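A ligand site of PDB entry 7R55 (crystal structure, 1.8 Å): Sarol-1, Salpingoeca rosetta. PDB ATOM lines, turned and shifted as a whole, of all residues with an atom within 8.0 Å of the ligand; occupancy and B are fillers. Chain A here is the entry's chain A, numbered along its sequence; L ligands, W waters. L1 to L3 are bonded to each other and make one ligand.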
ATOM      1  N   LYS A  91      17.586   1.851   4.692  1.00  0.00           N
ATOM      2  CA  LYS A  91      16.844   1.411   3.520  1.00  0.00           C
ATOM      3  C   LYS A  91      17.738   1.260   2.281  1.00  0.00           C
ATOM      4  O   LYS A  91      18.328   2.220   1.849  1.00  0.00           O
ATOM      5  CB  LYS A  91      15.816   2.485   3.184  1.00  0.00           C
ATOM      6  CG  LYS A  91      14.764   1.981   2.242  1.00  0.00           C
ATOM      7  CD  LYS A  91      13.419   2.666   2.529  1.00  0.00           C
ATOM      8  CE  LYS A  91      13.580   4.170   2.584  1.00  0.00           C
ATOM      9  NZ  LYS A  91      12.263   4.838   2.456  1.00  0.00           N
ATOM     10  N   GLU A  92      17.698   0.100   1.642  1.00  0.00           N
ATOM     11  CA  GLU A  92      18.340  -0.236   0.355  1.00  0.00           C
ATOM     12  C   GLU A  92      19.856  -0.155   0.487  1.00  0.00           C
ATOM     13  O   GLU A  92      20.517  -0.108  -0.557  1.00  0.00           O
ATOM     14  CB  GLU A  92      17.834   0.672  -0.776  1.00  0.00           C
ATOM     15  CG  GLU A  92      16.425   0.338  -1.237  1.00  0.00           C
ATOM     16  CD  GLU A  92      16.308  -0.956  -2.027  1.00  0.00           C
ATOM     17  OE1 GLU A  92      17.367  -1.494  -2.454  1.00  0.00           O
ATOM     18  OE2 GLU A  92      15.191  -1.446  -2.220  1.00  0.00           O
ATOM     19  N   TYR A 127      15.839  -6.106   7.794  1.00  0.00           N
ATOM     20  CA  TYR A 127      16.184  -7.491   7.429  1.00  0.00           C
ATOM     21  C   TYR A 127      16.818  -7.510   6.047  1.00  0.00           C
ATOM     22  O   TYR A 127      16.905  -6.493   5.359  1.00  0.00           O
ATOM     23  CB  TYR A 127      14.899  -8.288   7.389  1.00  0.00           C
ATOM     24  CG  TYR A 127      14.236  -8.487   8.725  1.00  0.00           C
ATOM     25  CD1 TYR A 127      13.510  -7.453   9.308  1.00  0.00           C
ATOM     26  CD2 TYR A 127      14.304  -9.707   9.368  1.00  0.00           C
ATOM     27  CE1 TYR A 127      12.958  -7.629  10.573  1.00  0.00           C
ATOM     28  CE2 TYR A 127      13.768  -9.876  10.627  1.00  0.00           C
ATOM     29  CZ  TYR A 127      12.990  -8.855  11.182  1.00  0.00           C
ATOM     30  OH  TYR A 127      12.512  -9.035  12.420  1.00  0.00           O
ATOM     31  N   VAL A 128      17.328  -8.673   5.640  1.00  0.00           N
ATOM     32  CA  VAL A 128      18.025  -8.806   4.358  1.00  0.00           C
ATOM     33  C   VAL A 128      16.983  -9.244   3.316  1.00  0.00           C
ATOM     34  O   VAL A 128      16.355 -10.285   3.507  1.00  0.00           O
ATOM     35  CB  VAL A 128      19.199  -9.763   4.479  1.00  0.00           C
ATOM     36  CG1 VAL A 128      19.849  -9.978   3.146  1.00  0.00           C
ATOM     37  CG2 VAL A 128      20.177  -9.225   5.522  1.00  0.00           C
ATOM     38  N   HIS A 129      16.843  -8.430   2.285  1.00  0.00           N
ATOM     39  CA  HIS A 129      15.961  -8.638   1.110  1.00  0.00           C
ATOM     40  C   HIS A 129      16.826  -8.693  -0.167  1.00  0.00           C
ATOM     41  O   HIS A 129      17.873  -8.053  -0.260  1.00  0.00           O
ATOM     42  CB  HIS A 129      14.984  -7.440   0.911  1.00  0.00           C
ATOM     43  CG  HIS A 129      14.063  -7.126   2.044  1.00  0.00           C
ATOM     44  ND1 HIS A 129      12.731  -6.768   1.835  1.00  0.00           N
ATOM     45  CD2 HIS A 129      14.257  -7.046   3.383  1.00  0.00           C
ATOM     46  CE1 HIS A 129      12.144  -6.571   3.006  1.00  0.00           C
ATOM     47  NE2 HIS A 129      13.068  -6.733   3.972  1.00  0.00           N
ATOM     48  N   PRO A 130      16.392  -9.444  -1.181  1.00  0.00           N
ATOM     49  CA  PRO A 130      16.892  -9.285  -2.533  1.00  0.00           C
ATOM     50  C   PRO A 130      16.408  -7.901  -2.986  1.00  0.00           C
ATOM     51  O   PRO A 130      15.214  -7.589  -2.838  1.00  0.00           O
ATOM     52  CB  PRO A 130      16.246 -10.410  -3.352  1.00  0.00           C
ATOM     53  CG  PRO A 130      15.485 -11.258  -2.355  1.00  0.00           C
ATOM     54  CD  PRO A 130      15.314 -10.447  -1.100  1.00  0.00           C
ATOM     55  N   HIS A 131      17.276  -7.103  -3.534  1.00  0.00           N
ATOM     56  CA  HIS A 131      16.896  -5.804  -4.115  1.00  0.00           C
ATOM     57  C   HIS A 131      15.759  -6.040  -5.134  1.00  0.00           C
ATOM     58  O   HIS A 131      15.919  -6.879  -6.021  1.00  0.00           O
ATOM     59  CB  HIS A 131      18.079  -5.151  -4.824  1.00  0.00           C
ATOM     60  CG  HIS A 131      17.675  -3.925  -5.530  1.00  0.00           C
ATOM     61  ND1 HIS A 131      17.238  -2.822  -4.851  1.00  0.00           N
ATOM     62  CD2 HIS A 131      17.591  -3.664  -6.874  1.00  0.00           C
ATOM     63  CE1 HIS A 131      16.953  -1.840  -5.734  1.00  0.00           C
ATOM     64  NE2 HIS A 131      17.185  -2.330  -7.006  1.00  0.00           N
ATOM     65  N   GLY A 132      14.668  -5.301  -5.024  1.00  0.00           N
ATOM     66  CA  GLY A 132      13.485  -5.472  -5.934  1.00  0.00           C
ATOM     67  C   GLY A 132      12.423  -6.281  -5.258  1.00  0.00           C
ATOM     68  O   GLY A 132      11.229  -6.222  -5.725  1.00  0.00           O
ATOM     69  N   GLY A 133      12.841  -7.131  -4.298  1.00  0.00           N
ATOM     70  CA  GLY A 133      11.916  -7.871  -3.426  1.00  0.00           C
ATOM     71  C   GLY A 133      11.175  -9.028  -4.085  1.00  0.00           C
ATOM     72  O   GLY A 133      10.190  -9.507  -3.469  1.00  0.00           O
ATOM     73  N   SER A 134      11.648  -9.519  -5.232  1.00  0.00           N
ATOM     74  CA  SER A 134      11.155 -10.742  -5.889  1.00  0.00           C
ATOM     75  C   SER A 134      11.243 -11.954  -4.968  1.00  0.00           C
ATOM     76  O   SER A 134      12.198 -12.156  -4.225  1.00  0.00           O
ATOM     77  CB  SER A 134      11.861 -11.078  -7.148  1.00  0.00           C
ATOM     78  OG  SER A 134      11.207 -12.241  -7.679  1.00  0.00           O
ATOM     79  N   THR A 141      21.276 -10.978  -8.358  1.00  0.00           N
ATOM     80  CA  THR A 141      20.456 -10.001  -7.632  1.00  0.00           C
ATOM     81  C   THR A 141      21.142  -9.670  -6.337  1.00  0.00           C
ATOM     82  O   THR A 141      21.458 -10.586  -5.590  1.00  0.00           O
ATOM     83  CB  THR A 141      19.037 -10.496  -7.363  1.00  0.00           C
ATOM     84  OG1 THR A 141      18.437 -10.812  -8.646  1.00  0.00           O
ATOM     85  CG2 THR A 141      18.263  -9.438  -6.623  1.00  0.00           C
ATOM     86  N   ARG A 142      21.393  -8.392  -6.081  1.00  0.00           N
ATOM     87  CA  ARG A 142      22.128  -7.980  -4.855  1.00  0.00           C
ATOM     88  C   ARG A 142      21.206  -8.087  -3.623  1.00  0.00           C
ATOM     89  O   ARG A 142      19.993  -7.969  -3.754  1.00  0.00           O
ATOM     90  CB  ARG A 142      22.764  -6.600  -5.015  1.00  0.00           C
ATOM     91  CG  ARG A 142      21.813  -5.461  -5.349  1.00  0.00           C
ATOM     92  CD  ARG A 142      22.507  -4.467  -6.288  1.00  0.00           C
ATOM     93  NE  ARG A 142      21.552  -3.427  -6.605  1.00  0.00           N
ATOM     94  CZ  ARG A 142      21.158  -2.551  -5.704  1.00  0.00           C
ATOM     95  NH1 ARG A 142      21.708  -2.592  -4.496  1.00  0.00           N
ATOM     96  NH2 ARG A 142      20.280  -1.623  -6.023  1.00  0.00           N
ATOM     97  N   LEU A 143      21.815  -8.291  -2.460  1.00  0.00           N
ATOM     98  CA  LEU A 143      21.112  -8.336  -1.150  1.00  0.00           C
ATOM     99  C   LEU A 143      21.232  -6.936  -0.551  1.00  0.00           C
ATOM    100  O   LEU A 143      22.329  -6.291  -0.688  1.00  0.00           O
ATOM    101  CB  LEU A 143      21.759  -9.379  -0.242  1.00  0.00           C
ATOM    102  CG  LEU A 143      21.616 -10.828  -0.681  1.00  0.00           C
ATOM    103  CD1 LEU A 143      22.223 -11.774   0.341  1.00  0.00           C
ATOM    104  CD2 LEU A 143      20.145 -11.186  -0.941  1.00  0.00           C
ATOM    105  N   VAL A 144      20.137  -6.460   0.020  1.00  0.00           N
ATOM    106  CA  VAL A 144      20.039  -5.117   0.637  1.00  0.00           C
ATOM    107  C   VAL A 144      19.334  -5.208   1.974  1.00  0.00           C
ATOM    108  O   VAL A 144      18.599  -6.156   2.238  1.00  0.00           O
ATOM    109  CB  VAL A 144      19.321  -4.108  -0.267  1.00  0.00           C
ATOM    110  CG1 VAL A 144      19.973  -3.964  -1.617  1.00  0.00           C
ATOM    111  CG2 VAL A 144      17.850  -4.471  -0.427  1.00  0.00           C
ATOM    112  N   TYR A 145      19.603  -4.252   2.833  1.00  0.00           N
ATOM    113  CA  TYR A 145      18.802  -4.094   4.054  1.00  0.00           C
ATOM    114  C   TYR A 145      17.520  -3.367   3.648  1.00  0.00           C
ATOM    115  O   TYR A 145      17.603  -2.439   2.937  1.00  0.00           O
ATOM    116  CB  TYR A 145      19.574  -3.361   5.090  1.00  0.00           C
ATOM    117  CG  TYR A 145      20.700  -4.154   5.702  1.00  0.00           C
ATOM    118  CD1 TYR A 145      20.391  -5.261   6.476  1.00  0.00           C
ATOM    119  CD2 TYR A 145      22.016  -3.903   5.412  1.00  0.00           C
ATOM    120  CE1 TYR A 145      21.363  -6.033   7.071  1.00  0.00           C
ATOM    121  CE2 TYR A 145      23.027  -4.660   6.038  1.00  0.00           C
ATOM    122  CZ  TYR A 145      22.687  -5.741   6.822  1.00  0.00           C
ATOM    123  OH  TYR A 145      23.572  -6.584   7.471  1.00  0.00           O
ATOM    124  N   TYR A 146      16.417  -3.717   4.272  1.00  0.00           N
ATOM    125  CA  TYR A 146      15.107  -3.083   4.098  1.00  0.00           C
ATOM    126  C   TYR A 146      14.280  -3.452   5.314  1.00  0.00           C
ATOM    127  O   TYR A 146      14.425  -4.530   5.934  1.00  0.00           O
ATOM    128  CB  TYR A 146      14.478  -3.591   2.822  1.00  0.00           C
ATOM    129  CG  TYR A 146      13.491  -2.649   2.237  1.00  0.00           C
ATOM    130  CD1 TYR A 146      12.163  -2.647   2.657  1.00  0.00           C
ATOM    131  CD2 TYR A 146      13.865  -1.767   1.221  1.00  0.00           C
ATOM    132  CE1 TYR A 146      11.251  -1.770   2.090  1.00  0.00           C
ATOM    133  CE2 TYR A 146      12.940  -0.934   0.599  1.00  0.00           C
ATOM    134  CZ  TYR A 146      11.635  -0.919   1.078  1.00  0.00           C
ATOM    135  OH  TYR A 146      10.727  -0.070   0.486  1.00  0.00           O
ATOM    136  N   SER A 147      13.409  -2.522   5.682  1.00  0.00           N
ATOM    137  CA  SER A 147      12.554  -2.648   6.864  1.00  0.00           C
ATOM    138  C   SER A 147      11.570  -3.786   6.706  1.00  0.00           C
ATOM    139  O   SER A 147      10.901  -3.905   5.634  1.00  0.00           O
ATOM    140  CB  SER A 147      11.801  -1.340   7.098  1.00  0.00           C
ATOM    141  OG  SER A 147      11.083  -1.499   8.327  1.00  0.00           O
ATOM    142  N   GLY A 148      11.397  -4.597   7.750  1.00  0.00           N
ATOM    143  CA  GLY A 148      10.311  -5.606   7.768  1.00  0.00           C
ATOM    144  C   GLY A 148      10.712  -6.928   7.149  1.00  0.00           C
ATOM    145  O   GLY A 148      11.715  -7.019   6.385  1.00  0.00           O
ATOM    146  N   TYR A 149       9.946  -7.951   7.394  1.00  0.00           N
ATOM    147  CA  TYR A 149      10.171  -9.276   6.777  1.00  0.00           C
ATOM    148  C   TYR A 149       8.853  -9.839   6.226  1.00  0.00           C
ATOM    149  O   TYR A 149       7.782  -9.405   6.606  1.00  0.00           O
ATOM    150  CB  TYR A 149      10.801 -10.183   7.838  1.00  0.00           C
ATOM    151  CG  TYR A 149       9.894 -10.616   8.940  1.00  0.00           C
ATOM    152  CD1 TYR A 149       9.106 -11.766   8.846  1.00  0.00           C
ATOM    153  CD2 TYR A 149       9.832  -9.897  10.121  1.00  0.00           C
ATOM    154  CE1 TYR A 149       8.279 -12.170   9.890  1.00  0.00           C
ATOM    155  CE2 TYR A 149       9.081 -10.331  11.198  1.00  0.00           C
ATOM    156  CZ  TYR A 149       8.268 -11.438  11.063  1.00  0.00           C
ATOM    157  OH  TYR A 149       7.476 -11.770  12.118  1.00  0.00           O
ATOM    158  N   ARG A 150       8.987 -10.871   5.422  1.00  0.00           N
ATOM    159  CA  ARG A 150       7.903 -11.700   4.895  1.00  0.00           C
ATOM    160  C   ARG A 150       8.485 -13.059   4.523  1.00  0.00           C
ATOM    161  O   ARG A 150       9.704 -13.183   4.391  1.00  0.00           O
ATOM    162  CB  ARG A 150       7.233 -10.984   3.725  1.00  0.00           C
ATOM    163  CG  ARG A 150       8.138 -10.828   2.516  1.00  0.00           C
ATOM    164  CD  ARG A 150       7.387 -10.084   1.420  1.00  0.00           C
ATOM    165  NE  ARG A 150       8.275  -9.671   0.313  1.00  0.00           N
ATOM    166  CZ  ARG A 150       8.973  -8.527   0.267  1.00  0.00           C
ATOM    167  NH1 ARG A 150       8.944  -7.653   1.261  1.00  0.00           N
ATOM    168  NH2 ARG A 150       9.685  -8.281  -0.785  1.00  0.00           N
ATOM    169  N   SER A 152       8.942 -14.975   1.886  1.00  0.00           N
ATOM    170  CA  SER A 152       9.820 -15.139   0.714  1.00  0.00           C
ATOM    171  C   SER A 152      11.273 -14.727   1.018  1.00  0.00           C
ATOM    172  O   SER A 152      12.140 -15.080   0.230  1.00  0.00           O
ATOM    173  CB  SER A 152       9.395 -14.329  -0.445  1.00  0.00           C
ATOM    174  OG  SER A 152       9.704 -12.981  -0.212  1.00  0.00           O
ATOM    175  N   LEU A 153      11.530 -13.989   2.074  1.00  0.00           N
ATOM    176  CA  LEU A 153      12.896 -13.511   2.438  1.00  0.00           C
ATOM    177  C   LEU A 153      13.675 -14.526   3.260  1.00  0.00           C
ATOM    178  O   LEU A 153      14.854 -14.222   3.563  1.00  0.00           O
ATOM    179  CB  LEU A 153      12.793 -12.206   3.222  1.00  0.00           C
ATOM    180  CG  LEU A 153      11.881 -11.102   2.691  1.00  0.00           C
ATOM    181  CD1 LEU A 153      11.914  -9.860   3.605  1.00  0.00           C
ATOM    182  CD2 LEU A 153      12.337 -10.656   1.306  1.00  0.00           C
HETATM  183  C1  LIG L   1      12.256   5.380  -1.566  1.00  0.00           C
HETATM  184  C2  LIG L   1      11.100   4.616  -0.951  1.00  0.00           C
HETATM  185  C3  LIG L   1      11.346   3.110  -1.021  1.00  0.00           C
HETATM  186  C4  LIG L   1      11.779   2.671  -2.380  1.00  0.00           C
HETATM  187  C5  LIG L   1      12.930   3.503  -2.934  1.00  0.00           C
HETATM  188  C6  LIG L   1      13.331   3.178  -4.387  1.00  0.00           C
HETATM  189  O1  LIG L   1      13.426   5.144  -0.789  1.00  0.00           O
HETATM  190  O2  LIG L   1      10.898   5.023   0.415  1.00  0.00           O
HETATM  191  O3  LIG L   1      10.081   2.559  -0.749  1.00  0.00           O
HETATM  192  O4  LIG L   1      12.253   1.347  -2.342  1.00  0.00           O
HETATM  193  O5  LIG L   1      12.503   4.893  -2.902  1.00  0.00           O
HETATM  194  O6  LIG L   1      14.720   3.591  -4.463  1.00  0.00           O
HETATM  195  C1  LG2 L   2      11.589   0.642  -3.308  1.00  0.00           C
HETATM  196  C2  LG2 L   2      12.434  -0.593  -3.545  1.00  0.00           C
HETATM  197  C3  LG2 L   2      11.743  -1.486  -4.564  1.00  0.00           C
HETATM  198  C4  LG2 L   2      10.340  -1.829  -4.103  1.00  0.00           C
HETATM  199  C5  LG2 L   2       9.596  -0.540  -3.785  1.00  0.00           C
HETATM  200  C6  LG2 L   2       8.200  -0.862  -3.241  1.00  0.00           C
HETATM  201  O1  LG2 L   2      13.667  -0.211  -4.039  1.00  0.00           O
HETATM  202  O2  LG2 L   2      12.518  -2.684  -4.845  1.00  0.00           O
HETATM  203  O3  LG2 L   2      10.293  -2.531  -2.870  1.00  0.00           O
HETATM  204  O4  LG2 L   2      10.252   0.336  -2.842  1.00  0.00           O
HETATM  205  O5  LG2 L   2       7.719   0.490  -3.133  1.00  0.00           O
HETATM  206  C1  LG3 L   3      10.469  -3.939  -3.027  1.00  0.00           C
HETATM  207  C2  LG3 L   3       9.607  -4.587  -1.901  1.00  0.00           C
HETATM  208  C3  LG3 L   3      10.209  -4.283  -0.504  1.00  0.00           C
HETATM  209  C4  LG3 L   3      11.660  -4.744  -0.444  1.00  0.00           C
HETATM  210  C5  LG3 L   3      12.378  -4.094  -1.623  1.00  0.00           C
HETATM  211  C6  LG3 L   3      13.872  -4.471  -1.661  1.00  0.00           C
HETATM  212  O1  LG3 L   3       8.238  -4.145  -2.038  1.00  0.00           O
HETATM  213  O2  LG3 L   3       9.405  -4.946   0.431  1.00  0.00           O
HETATM  214  O3  LG3 L   3      11.699  -6.176  -0.508  1.00  0.00           O
HETATM  215  O4  LG3 L   3      11.836  -4.375  -2.869  1.00  0.00           O
HETATM  216  O5  LG3 L   3      14.500  -3.804  -2.731  1.00  0.00           O
HETATM  217  O   HOH W   1      14.106  -1.721  -6.878  1.00  0.00           O
HETATM  218  O   HOH W   2       6.437  -6.139  -0.854  1.00  0.00           O
HETATM  219  O   HOH W   3       7.965  -3.719   2.242  1.00  0.00           O
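An oxygen (O2) of LIG L1 sits at hydrogen-bond distance from the side-chain amino group (NZ) of Lys 91, 2.5 Å away.
OE2 of Glu 92 lies within hydrogen-bond range of O5 of LG3 L3 (2.5 Å).
ND1 of His 129 sits at hydrogen-bond distance from O3 of LG3 L3.
N of Gly 132 is in hydrogen-bond range of O5 of LG3 L3 (2.7 Å).
The guanidinium group (NH1) of Arg 150 sits at hydrogen-bond distance from an oxygen (O2) of LG3 L3 (2.9 Å).
OH of Tyr 146 lies within hydrogen-bond range of O3 of LIG L1.
The backbone NH of Gly 133 is in hydrogen-bond range of an oxygen (O4) of LG3 L3 (3.3 Å).
Water W1 bridges O2 of LG2 L2 (2.8 Å) and NE2 of His 131 (3.1 Å).
The side-chain carboxylate (OE1) of Glu 92 lies within hydrogen-bond range of a ring nitrogen (ND1) of His 131.
O of Tyr 145 sits at hydrogen-bond distance from N of Glu 92, 2.9 Å away.
A ring nitrogen (NE2) of His 129 is in hydrogen-bond range of the backbone carbonyl oxygen of Tyr 146 (3.2 Å).
O of His 129 sits at hydrogen-bond distance from N of Val 144, 2.8 Å away.
A ring nitrogen (NE2) of His 129 lies within hydrogen-bond range of the backbone carbonyl oxygen (O) of Gly 148 (2.8 Å).
O of Gly 133 sits at hydrogen-bond distance from NH2 of Arg 150, 3.0 Å away.
N of Tyr 127 sits at hydrogen-bond distance from O of Tyr 146, at 2.8 Å.
N of His 131 sits at hydrogen-bond distance from O of Arg 142 (2.9 Å).
Merely in contact with the ligand: His 131 and Pro 130.
Within 4 Å of the ligand: Lys 91, Glu 92, His 129, Pro 130, His 131, Gly 132, Gly 133, Tyr 146 and Arg 150.
The nearest printed residue that does not touch the ligand is Val 144 (4.1 Å).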
